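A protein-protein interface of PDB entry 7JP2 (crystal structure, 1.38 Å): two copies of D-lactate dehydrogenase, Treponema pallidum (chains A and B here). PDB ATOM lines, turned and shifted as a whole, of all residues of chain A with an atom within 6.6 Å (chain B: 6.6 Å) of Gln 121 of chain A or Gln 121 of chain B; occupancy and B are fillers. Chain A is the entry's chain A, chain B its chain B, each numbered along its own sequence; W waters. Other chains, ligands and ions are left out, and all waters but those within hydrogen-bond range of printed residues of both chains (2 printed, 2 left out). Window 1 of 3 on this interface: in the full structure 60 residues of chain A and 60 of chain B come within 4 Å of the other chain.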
ATOM      1  N   TYR A 114       0.753 -13.245   2.911  1.00  0.00           N
ATOM      2  CA  TYR A 114       1.032 -12.788   4.265  1.00  0.00           C
ATOM      3  C   TYR A 114       2.392 -12.087   4.326  1.00  0.00           C
ATOM      4  O   TYR A 114       2.537 -11.039   4.969  1.00  0.00           O
ATOM      5  CB  TYR A 114       0.942 -13.919   5.314  1.00  0.00           C
ATOM      6  CG  TYR A 114       1.147 -13.272   6.655  1.00  0.00           C
ATOM      7  CD1 TYR A 114       2.386 -13.278   7.273  1.00  0.00           C
ATOM      8  CD2 TYR A 114       0.141 -12.509   7.223  1.00  0.00           C
ATOM      9  CE1 TYR A 114       2.603 -12.579   8.450  1.00  0.00           C
ATOM     10  CE2 TYR A 114       0.338 -11.816   8.391  1.00  0.00           C
ATOM     11  CZ  TYR A 114       1.569 -11.839   9.000  1.00  0.00           C
ATOM     12  OH  TYR A 114       1.758 -11.077  10.125  1.00  0.00           O
ATOM     13  N   LEU A 116       3.889 -10.389   2.013  1.00  0.00           N
ATOM     14  CA  LEU A 116       3.702  -9.055   1.453  1.00  0.00           C
ATOM     15  C   LEU A 116       2.923  -8.154   2.411  1.00  0.00           C
ATOM     16  O   LEU A 116       3.298  -6.993   2.630  1.00  0.00           O
ATOM     17  CB  LEU A 116       2.987  -9.155   0.101  1.00  0.00           C
ATOM     18  CG  LEU A 116       2.578  -7.804  -0.480  1.00  0.00           C
ATOM     19  CD1 LEU A 116       3.767  -6.905  -0.805  1.00  0.00           C
ATOM     20  CD2 LEU A 116       1.701  -7.981  -1.712  1.00  0.00           C
ATOM     21  N   ALA A 117       1.830  -8.673   2.983  1.00  0.00           N
ATOM     22  CA  ALA A 117       1.024  -7.906   3.928  1.00  0.00           C
ATOM     23  C   ALA A 117       1.854  -7.429   5.109  1.00  0.00           C
ATOM     24  O   ALA A 117       1.779  -6.260   5.511  1.00  0.00           O
ATOM     25  CB  ALA A 117      -0.133  -8.772   4.422  1.00  0.00           C
ATOM     26  N   ALA A 118       2.648  -8.332   5.684  1.00  0.00           N
ATOM     27  CA  ALA A 118       3.492  -7.989   6.820  1.00  0.00           C
ATOM     28  C   ALA A 118       4.583  -7.010   6.409  1.00  0.00           C
ATOM     29  O   ALA A 118       4.869  -6.046   7.128  1.00  0.00           O
ATOM     30  CB  ALA A 118       4.096  -9.262   7.406  1.00  0.00           C
ATOM     31  N   ALA A 119       5.184  -7.221   5.235  1.00  0.00           N
ATOM     32  CA  ALA A 119       6.192  -6.285   4.755  1.00  0.00           C
ATOM     33  C   ALA A 119       5.615  -4.885   4.634  1.00  0.00           C
ATOM     34  O   ALA A 119       6.252  -3.909   5.039  1.00  0.00           O
ATOM     35  CB  ALA A 119       6.750  -6.740   3.411  1.00  0.00           C
ATOM     36  N   LEU A 120       4.392  -4.772   4.104  1.00  0.00           N
ATOM     37  CA  LEU A 120       3.769  -3.459   3.967  1.00  0.00           C
ATOM     38  C   LEU A 120       3.378  -2.858   5.317  1.00  0.00           C
ATOM     39  O   LEU A 120       3.425  -1.631   5.479  1.00  0.00           O
ATOM     40  CB  LEU A 120       2.558  -3.532   3.036  1.00  0.00           C
ATOM     41  CG  LEU A 120       2.884  -3.567   1.541  1.00  0.00           C
ATOM     42  CD1 LEU A 120       1.671  -4.015   0.726  1.00  0.00           C
ATOM     43  CD2 LEU A 120       3.373  -2.206   1.071  1.00  0.00           C
ATOM     44  N   GLN A 121       3.002  -3.679   6.300  1.00  0.00           N
ATOM     45  CA  GLN A 121       2.827  -3.136   7.646  1.00  0.00           C
ATOM     46  C   GLN A 121       4.111  -2.475   8.133  1.00  0.00           C
ATOM     47  O   GLN A 121       4.077  -1.431   8.794  1.00  0.00           O
ATOM     48  CB  GLN A 121       2.426  -4.233   8.634  1.00  0.00           C
ATOM     49  CG  GLN A 121       0.982  -4.649   8.574  1.00  0.00           C
ATOM     50  CD  GLN A 121       0.677  -5.671   9.636  1.00  0.00           C
ATOM     51  OE1 GLN A 121       0.909  -5.431  10.824  1.00  0.00           O
ATOM     52  NE2 GLN A 121       0.187  -6.829   9.223  1.00  0.00           N
ATOM     53  N   LEU A 122       5.259  -3.081   7.812  1.00  0.00           N
ATOM     54  CA  LEU A 122       6.543  -2.533   8.229  1.00  0.00           C
ATOM     55  C   LEU A 122       6.915  -1.307   7.404  1.00  0.00           C
ATOM     56  O   LEU A 122       7.235  -0.251   7.955  1.00  0.00           O
ATOM     57  CB  LEU A 122       7.621  -3.617   8.132  1.00  0.00           C
ATOM     58  CG  LEU A 122       7.438  -4.797   9.095  1.00  0.00           C
ATOM     59  CD1 LEU A 122       8.391  -5.934   8.767  1.00  0.00           C
ATOM     60  CD2 LEU A 122       7.588  -4.350  10.543  1.00  0.00           C
ATOM     61  N   THR A 123       6.895  -1.427   6.073  1.00  0.00           N
ATOM     62  CA  THR A 123       7.419  -0.335   5.261  1.00  0.00           C
ATOM     63  C   THR A 123       6.511   0.884   5.275  1.00  0.00           C
ATOM     64  O   THR A 123       6.983   2.001   5.050  1.00  0.00           O
ATOM     65  CB  THR A 123       7.654  -0.769   3.812  1.00  0.00           C
ATOM     66  OG1 THR A 123       6.414  -1.167   3.213  1.00  0.00           O
ATOM     67  CG2 THR A 123       8.674  -1.887   3.731  1.00  0.00           C
ATOM     68  N   ARG A 124       5.219   0.699   5.510  1.00  0.00           N
ATOM     69  CA  ARG A 124       4.279   1.805   5.625  1.00  0.00           C
ATOM     70  C   ARG A 124       4.055   2.236   7.074  1.00  0.00           C
ATOM     71  O   ARG A 124       3.167   3.050   7.346  1.00  0.00           O
ATOM     72  CB  ARG A 124       2.978   1.477   4.899  1.00  0.00           C
ATOM     73  CG  ARG A 124       3.180   1.229   3.400  1.00  0.00           C
ATOM     74  CD  ARG A 124       3.835   2.439   2.660  1.00  0.00           C
ATOM     75  NE  ARG A 124       3.064   3.675   2.822  1.00  0.00           N
ATOM     76  CZ  ARG A 124       2.419   4.329   1.855  1.00  0.00           C
ATOM     77  NH1 ARG A 124       2.466   3.932   0.589  1.00  0.00           N
ATOM     78  NH2 ARG A 124       1.733   5.415   2.163  1.00  0.00           N
ATOM     79  N   HIS A 125       4.866   1.738   8.001  1.00  0.00           N
ATOM     80  CA  HIS A 125       4.913   2.252   9.370  1.00  0.00           C
ATOM     81  C   HIS A 125       3.577   2.133  10.099  1.00  0.00           C
ATOM     82  O   HIS A 125       3.211   3.007  10.886  1.00  0.00           O
ATOM     83  CB  HIS A 125       5.413   3.702   9.409  1.00  0.00           C
ATOM     84  CG  HIS A 125       6.807   3.863   8.901  1.00  0.00           C
ATOM     85  ND1 HIS A 125       7.916   3.710   9.701  1.00  0.00           N
ATOM     86  CD2 HIS A 125       7.270   4.120   7.659  1.00  0.00           C
ATOM     87  CE1 HIS A 125       9.005   3.888   8.974  1.00  0.00           C
ATOM     88  NE2 HIS A 125       8.640   4.129   7.731  1.00  0.00           N
ATOM     89  N   ALA A 126       2.861   1.029   9.883  1.00  0.00           N
ATOM     90  CA  ALA A 126       1.518   0.915  10.448  1.00  0.00           C
ATOM     91  C   ALA A 126       1.522   1.054  11.971  1.00  0.00           C
ATOM     92  O   ALA A 126       0.692   1.771  12.541  1.00  0.00           O
ATOM     93  CB  ALA A 126       0.873  -0.404  10.022  1.00  0.00           C
ATOM     94  N   ARG A 127       2.424   0.350  12.650  1.00  0.00           N
ATOM     95  CA  ARG A 127       2.412   0.372  14.111  1.00  0.00           C
ATOM     96  C   ARG A 127       2.829   1.734  14.651  1.00  0.00           C
ATOM     97  O   ARG A 127       2.238   2.234  15.608  1.00  0.00           O
ATOM     98  CB  ARG A 127       3.316  -0.729  14.655  1.00  0.00           C
ATOM     99  CG  ARG A 127       3.429  -0.717  16.161  1.00  0.00           C
ATOM    100  CD  ARG A 127       4.143  -1.952  16.674  1.00  0.00           C
ATOM    101  NE  ARG A 127       3.319  -3.141  16.497  1.00  0.00           N
ATOM    102  CZ  ARG A 127       3.744  -4.373  16.733  1.00  0.00           C
ATOM    103  NH1 ARG A 127       4.978  -4.563  17.159  1.00  0.00           N
ATOM    104  NH2 ARG A 127       2.933  -5.410  16.559  1.00  0.00           N
ATOM    105  N   GLU A 128       3.836   2.355  14.039  1.00  0.00           N
ATOM    106  CA  GLU A 128       4.280   3.666  14.495  1.00  0.00           C
ATOM    107  C   GLU A 128       3.190   4.708  14.284  1.00  0.00           C
ATOM    108  O   GLU A 128       2.970   5.569  15.148  1.00  0.00           O
ATOM    109  CB  GLU A 128       5.569   4.048  13.778  1.00  0.00           C
ATOM    110  CG  GLU A 128       6.686   3.050  14.006  1.00  0.00           C
ATOM    111  CD  GLU A 128       6.899   2.108  12.831  1.00  0.00           C
ATOM    112  OE1 GLU A 128       5.931   1.474  12.331  1.00  0.00           O
ATOM    113  OE2 GLU A 128       8.071   2.015  12.404  1.00  0.00           O
ATOM    114  N   ILE A 297       6.189  -7.701  14.701  1.00  0.00           N
ATOM    115  CA  ILE A 297       4.798  -8.075  14.461  1.00  0.00           C
ATOM    116  C   ILE A 297       4.782  -9.596  14.579  1.00  0.00           C
ATOM    117  O   ILE A 297       5.198 -10.309  13.655  1.00  0.00           O
ATOM    118  CB  ILE A 297       4.310  -7.619  13.087  1.00  0.00           C
ATOM    119  CG1 ILE A 297       4.458  -6.110  12.917  1.00  0.00           C
ATOM    120  CG2 ILE A 297       2.849  -8.023  12.899  1.00  0.00           C
ATOM    121  CD1 ILE A 297       4.299  -5.652  11.481  1.00  0.00           C
ATOM    122  N   THR A 299       2.948 -13.145  14.947  1.00  0.00           N
ATOM    123  CA  THR A 299       1.700 -13.828  14.667  1.00  0.00           C
ATOM    124  C   THR A 299       1.857 -15.325  14.877  1.00  0.00           C
ATOM    125  O   THR A 299       2.952 -15.876  14.705  1.00  0.00           O
ATOM    126  CB  THR A 299       1.225 -13.540  13.238  1.00  0.00           C
ATOM    127  OG1 THR A 299       2.268 -13.800  12.296  1.00  0.00           O
ATOM    128  CG2 THR A 299       0.813 -12.091  13.077  1.00  0.00           C
ATOM    129  N   TYR B 114      -0.764   2.405  -0.371  1.00  0.00           N
ATOM    130  CA  TYR B 114      -1.385   2.467   0.947  1.00  0.00           C
ATOM    131  C   TYR B 114      -2.746   1.766   0.933  1.00  0.00           C
ATOM    132  O   TYR B 114      -3.091   1.034   1.869  1.00  0.00           O
ATOM    133  CB  TYR B 114      -1.496   3.904   1.508  1.00  0.00           C
ATOM    134  CG  TYR B 114      -2.044   3.785   2.916  1.00  0.00           C
ATOM    135  CD1 TYR B 114      -3.392   3.958   3.185  1.00  0.00           C
ATOM    136  CD2 TYR B 114      -1.234   3.342   3.950  1.00  0.00           C
ATOM    137  CE1 TYR B 114      -3.907   3.740   4.463  1.00  0.00           C
ATOM    138  CE2 TYR B 114      -1.735   3.115   5.206  1.00  0.00           C
ATOM    139  CZ  TYR B 114      -3.067   3.302   5.456  1.00  0.00           C
ATOM    140  OH  TYR B 114      -3.549   3.022   6.714  1.00  0.00           O
ATOM    141  N   LEU B 116      -3.693  -0.750  -0.855  1.00  0.00           N
ATOM    142  CA  LEU B 116      -3.436  -2.184  -0.808  1.00  0.00           C
ATOM    143  C   LEU B 116      -2.949  -2.611   0.572  1.00  0.00           C
ATOM    144  O   LEU B 116      -3.405  -3.625   1.111  1.00  0.00           O
ATOM    145  CB  LEU B 116      -2.405  -2.552  -1.870  1.00  0.00           C
ATOM    146  CG  LEU B 116      -1.890  -3.988  -1.787  1.00  0.00           C
ATOM    147  CD1 LEU B 116      -3.021  -4.981  -2.013  1.00  0.00           C
ATOM    148  CD2 LEU B 116      -0.750  -4.218  -2.772  1.00  0.00           C
ATOM    149  N   ALA B 117      -2.018  -1.850   1.158  1.00  0.00           N
ATOM    150  CA  ALA B 117      -1.485  -2.186   2.472  1.00  0.00           C
ATOM    151  C   ALA B 117      -2.592  -2.223   3.513  1.00  0.00           C
ATOM    152  O   ALA B 117      -2.665  -3.142   4.339  1.00  0.00           O
ATOM    153  CB  ALA B 117      -0.430  -1.150   2.865  1.00  0.00           C
ATOM    154  N   ALA B 118      -3.455  -1.210   3.495  1.00  0.00           N
ATOM    155  CA  ALA B 118      -4.561  -1.142   4.437  1.00  0.00           C
ATOM    156  C   ALA B 118      -5.571  -2.254   4.181  1.00  0.00           C
ATOM    157  O   ALA B 118      -6.070  -2.877   5.127  1.00  0.00           O
ATOM    158  CB  ALA B 118      -5.226   0.231   4.336  1.00  0.00           C
ATOM    159  N   ALA B 119      -5.893  -2.511   2.912  1.00  0.00           N
ATOM    160  CA  ALA B 119      -6.783  -3.621   2.590  1.00  0.00           C
ATOM    161  C   ALA B 119      -6.244  -4.932   3.148  1.00  0.00           C
ATOM    162  O   ALA B 119      -7.005  -5.731   3.700  1.00  0.00           O
ATOM    163  CB  ALA B 119      -6.975  -3.721   1.076  1.00  0.00           C
ATOM    164  N   LEU B 120      -4.936  -5.177   3.006  1.00  0.00           N
ATOM    165  CA  LEU B 120      -4.356  -6.413   3.521  1.00  0.00           C
ATOM    166  C   LEU B 120      -4.341  -6.438   5.048  1.00  0.00           C
ATOM    167  O   LEU B 120      -4.477  -7.513   5.639  1.00  0.00           O
ATOM    168  CB  LEU B 120      -2.951  -6.636   2.959  1.00  0.00           C
ATOM    169  CG  LEU B 120      -2.920  -7.173   1.531  1.00  0.00           C
ATOM    170  CD1 LEU B 120      -1.509  -7.048   0.941  1.00  0.00           C
ATOM    171  CD2 LEU B 120      -3.400  -8.625   1.473  1.00  0.00           C
ATOM    172  N   GLN B 121      -4.189  -5.287   5.712  1.00  0.00           N
ATOM    173  CA  GLN B 121      -4.366  -5.286   7.163  1.00  0.00           C
ATOM    174  C   GLN B 121      -5.762  -5.766   7.536  1.00  0.00           C
ATOM    175  O   GLN B 121      -5.940  -6.478   8.530  1.00  0.00           O
ATOM    176  CB  GLN B 121      -4.136  -3.897   7.749  1.00  0.00           C
ATOM    177  CG  GLN B 121      -2.692  -3.481   7.866  1.00  0.00           C
ATOM    178  CD  GLN B 121      -2.570  -2.138   8.540  1.00  0.00           C
ATOM    179  OE1 GLN B 121      -3.084  -1.939   9.640  1.00  0.00           O
ATOM    180  NE2 GLN B 121      -1.927  -1.191   7.871  1.00  0.00           N
ATOM    181  N   LEU B 122      -6.768  -5.355   6.763  1.00  0.00           N
ATOM    182  CA  LEU B 122      -8.140  -5.779   7.020  1.00  0.00           C
ATOM    183  C   LEU B 122      -8.348  -7.245   6.654  1.00  0.00           C
ATOM    184  O   LEU B 122      -8.821  -8.039   7.478  1.00  0.00           O
ATOM    185  CB  LEU B 122      -9.088  -4.883   6.220  1.00  0.00           C
ATOM    186  CG  LEU B 122      -9.126  -3.411   6.628  1.00  0.00           C
ATOM    187  CD1 LEU B 122      -9.981  -2.610   5.633  1.00  0.00           C
ATOM    188  CD2 LEU B 122      -9.638  -3.214   8.057  1.00  0.00           C
ATOM    189  N   THR B 123      -8.018  -7.627   5.416  1.00  0.00           N
ATOM    190  CA  THR B 123      -8.391  -8.960   4.964  1.00  0.00           C
ATOM    191  C   THR B 123      -7.577 -10.043   5.664  1.00  0.00           C
ATOM    192  O   THR B 123      -8.040 -11.180   5.773  1.00  0.00           O
ATOM    193  CB  THR B 123      -8.247  -9.115   3.447  1.00  0.00           C
ATOM    194  OG1 THR B 123      -6.879  -8.922   3.075  1.00  0.00           O
ATOM    195  CG2 THR B 123      -9.127  -8.126   2.693  1.00  0.00           C
ATOM    196  N   ARG B 124      -6.359  -9.731   6.107  1.00  0.00           N
ATOM    197  CA  ARG B 124      -5.527 -10.680   6.839  1.00  0.00           C
ATOM    198  C   ARG B 124      -5.648 -10.516   8.354  1.00  0.00           C
ATOM    199  O   ARG B 124      -4.886 -11.138   9.101  1.00  0.00           O
ATOM    200  CB  ARG B 124      -4.071 -10.603   6.375  1.00  0.00           C
ATOM    201  CG  ARG B 124      -3.866 -10.973   4.905  1.00  0.00           C
ATOM    202  CD  ARG B 124      -4.407 -12.361   4.543  1.00  0.00           C
ATOM    203  NE  ARG B 124      -3.761 -13.413   5.318  1.00  0.00           N
ATOM    204  CZ  ARG B 124      -2.956 -14.356   4.838  1.00  0.00           C
ATOM    205  NH1 ARG B 124      -2.687 -14.455   3.540  1.00  0.00           N
ATOM    206  NH2 ARG B 124      -2.420 -15.227   5.683  1.00  0.00           N
ATOM    207  N   HIS B 125      -6.611  -9.724   8.822  1.00  0.00           N
ATOM    208  CA  HIS B 125      -7.001  -9.701  10.236  1.00  0.00           C
ATOM    209  C   HIS B 125      -5.862  -9.267  11.152  1.00  0.00           C
ATOM    210  O   HIS B 125      -5.713  -9.770  12.265  1.00  0.00           O
ATOM    211  CB  HIS B 125      -7.561 -11.060  10.671  1.00  0.00           C
ATOM    212  CG  HIS B 125      -8.817 -11.441   9.959  1.00  0.00           C
ATOM    213  ND1 HIS B 125     -10.068 -11.053  10.390  1.00  0.00           N
ATOM    214  CD2 HIS B 125      -9.013 -12.130   8.812  1.00  0.00           C
ATOM    215  CE1 HIS B 125     -10.982 -11.513   9.552  1.00  0.00           C
ATOM    216  NE2 HIS B 125     -10.366 -12.163   8.582  1.00  0.00           N
ATOM    217  N   ALA B 126      -5.082  -8.282  10.717  1.00  0.00           N
ATOM    218  CA  ALA B 126      -3.890  -7.918  11.479  1.00  0.00           C
ATOM    219  C   ALA B 126      -4.240  -7.511  12.909  1.00  0.00           C
ATOM    220  O   ALA B 126      -3.615  -7.974  13.868  1.00  0.00           O
ATOM    221  CB  ALA B 126      -3.123  -6.812  10.757  1.00  0.00           C
ATOM    222  N   ARG B 127      -5.209  -6.613  13.070  1.00  0.00           N
ATOM    223  CA  ARG B 127      -5.525  -6.110  14.405  1.00  0.00           C
ATOM    224  C   ARG B 127      -6.120  -7.202  15.289  1.00  0.00           C
ATOM    225  O   ARG B 127      -5.797  -7.293  16.480  1.00  0.00           O
ATOM    226  CB  ARG B 127      -6.502  -4.941  14.290  1.00  0.00           C
ATOM    227  CG  ARG B 127      -6.943  -4.400  15.631  1.00  0.00           C
ATOM    228  CD  ARG B 127      -7.797  -3.161  15.482  1.00  0.00           C
ATOM    229  NE  ARG B 127      -7.011  -2.023  15.013  1.00  0.00           N
ATOM    230  CZ  ARG B 127      -7.524  -0.835  14.725  1.00  0.00           C
ATOM    231  NH1 ARG B 127      -8.825  -0.622  14.840  1.00  0.00           N
ATOM    232  NH2 ARG B 127      -6.731   0.140  14.322  1.00  0.00           N
ATOM    233  N   GLU B 128      -6.997  -8.025  14.720  1.00  0.00           N
ATOM    234  CA  GLU B 128      -7.640  -9.093  15.471  1.00  0.00           C
ATOM    235  C   GLU B 128      -6.624 -10.131  15.927  1.00  0.00           C
ATOM    236  O   GLU B 128      -6.693 -10.621  17.062  1.00  0.00           O
ATOM    237  CB  GLU B 128      -8.730  -9.714  14.597  1.00  0.00           C
ATOM    238  CG  GLU B 128      -9.873  -8.743  14.231  1.00  0.00           C
ATOM    239  CD  GLU B 128      -9.486  -7.625  13.227  1.00  0.00           C
ATOM    240  OE1 GLU B 128      -8.602  -7.814  12.354  1.00  0.00           O
ATOM    241  OE2 GLU B 128     -10.078  -6.527  13.313  1.00  0.00           O
ATOM    242  N   ILE B 297      -9.159   1.289  11.014  1.00  0.00           N
ATOM    243  CA  ILE B 297      -7.740   1.631  10.978  1.00  0.00           C
ATOM    244  C   ILE B 297      -7.693   3.083  10.518  1.00  0.00           C
ATOM    245  O   ILE B 297      -7.840   3.373   9.329  1.00  0.00           O
ATOM    246  CB  ILE B 297      -6.948   0.722  10.038  1.00  0.00           C
ATOM    247  CG1 ILE B 297      -7.125  -0.747  10.409  1.00  0.00           C
ATOM    248  CG2 ILE B 297      -5.456   1.115  10.072  1.00  0.00           C
ATOM    249  CD1 ILE B 297      -6.599  -1.724   9.357  1.00  0.00           C
ATOM    250  N   THR B 299      -5.798   6.633   9.970  1.00  0.00           N
ATOM    251  CA  THR B 299      -4.486   7.214   9.753  1.00  0.00           C
ATOM    252  C   THR B 299      -4.648   8.675   9.355  1.00  0.00           C
ATOM    253  O   THR B 299      -5.663   9.054   8.755  1.00  0.00           O
ATOM    254  CB  THR B 299      -3.701   6.435   8.686  1.00  0.00           C
ATOM    255  OG1 THR B 299      -4.489   6.276   7.510  1.00  0.00           O
ATOM    256  CG2 THR B 299      -3.311   5.058   9.191  1.00  0.00           C
HETATM  257  O   HOH W   1       0.450  -1.163   6.185  1.00  0.00           O
HETATM  258  O   HOH W   2      -1.779  -7.574   7.210  1.00  0.00           O
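Of the 16 printed residues of chain A, 6 touch a printed residue of chain B.
Hydrophobic or aromatic side chains of chain A within 4 Å of the printed part of chain B: Tyr 114, Ala 117, Leu 120 and Ala 126.
Of the 16 printed residues of chain B, 6 touch a printed residue of chain A.
Printed residues of chain B that touch a printed residue of chain A: Tyr 114, Ala 117, Leu 120, Gln 121, Arg 124 and Ala 126.
Hydrophobic or aromatic side chains of chain B within 4 Å of the printed part of chain A: Tyr 114, Ala 117, Leu 120 and Ala 126.
Among the printed residues, 7 pairs touch across the chains.
Ala 119 of chain A touches none of the printed residues of chain B.
Of the printed residues of chain B, Gln 121 of chain A touches Gln 121 (3.9 Å) and Ala 126 (3.6 Å).
Leu 122 of chain A touches none of the printed residues of chain B.
Printed residues of chain B within 4 Å of Arg 124 of chain A: Tyr 114 (3.6 Å).
Of the printed residues of chain B, Ala 126 of chain A touches Gln 121 (3.6 Å).
Of the printed residues of chain A, Arg 124 of chain B touches Tyr 114 (3.6 Å).
Of the printed residues of chain A, Ala 126 of chain B touches Gln 121 (3.6 Å).
The nearest residue of chain B that does not touch Gln 121 of chain A is Ala 117 of chain B (5.5 Å).
Tyr 114 of chain A touches Arg 124 of chain B, and with the chains exchanged Arg 124 of chain A touches Tyr 114 of chain B.
Ala 117 of chain A touches Leu 120 of chain B, and with the chains exchanged Leu 120 of chain A touches Ala 117 of chain B.
Gln 121 of chain B touches its own counterpart, Gln 121 of chain A.
Gln 121 of chain A touches Ala 126 of chain B, and with the chains exchanged Ala 126 of chain A touches Gln 121 of chain B.
Of the 7 pairs that touch across the chains among the printed residues, 7 have their exchanged pair printed and touching as well.
Among the printed residues, pairs that only touch across the chains: Tyr 114 of chain A with Arg 124 of chain B, Ala 117 of chain A with Leu 120 of chain B, Leu 120 of chain A with Ala 117 of chain B, Gln 121 of chain A with Gln 121 of chain B, Gln 121 of chain A with Ala 126 of chain B, Arg 124 of chain A with Tyr 114 of chain B and Ala 126 of chain A with Gln 121 of chain B.
Water W2 lies within hydrogen-bond range of NE2 of Gln 121 of chain A and O of Leu 120 of chain B.
Water W1 bridges the side-chain amide nitrogen of Gln 121 of chain B and the backbone carbonyl oxygen of Leu 120 of chain A.
O of Gln 121 of chain B is in hydrogen-bond range of N of Ala 126 of chain B (3.0 Å).
The backbone carbonyl oxygen (O) of Gln 121 of chain A is in hydrogen-bond range of the backbone NH (N) of Ala 126 of chain A (3.0 Å).
The side-chain hydroxyl (OH) of Tyr 114 of chain B lies close to the side-chain hydroxyl (OG1) of Thr 299 of chain B.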
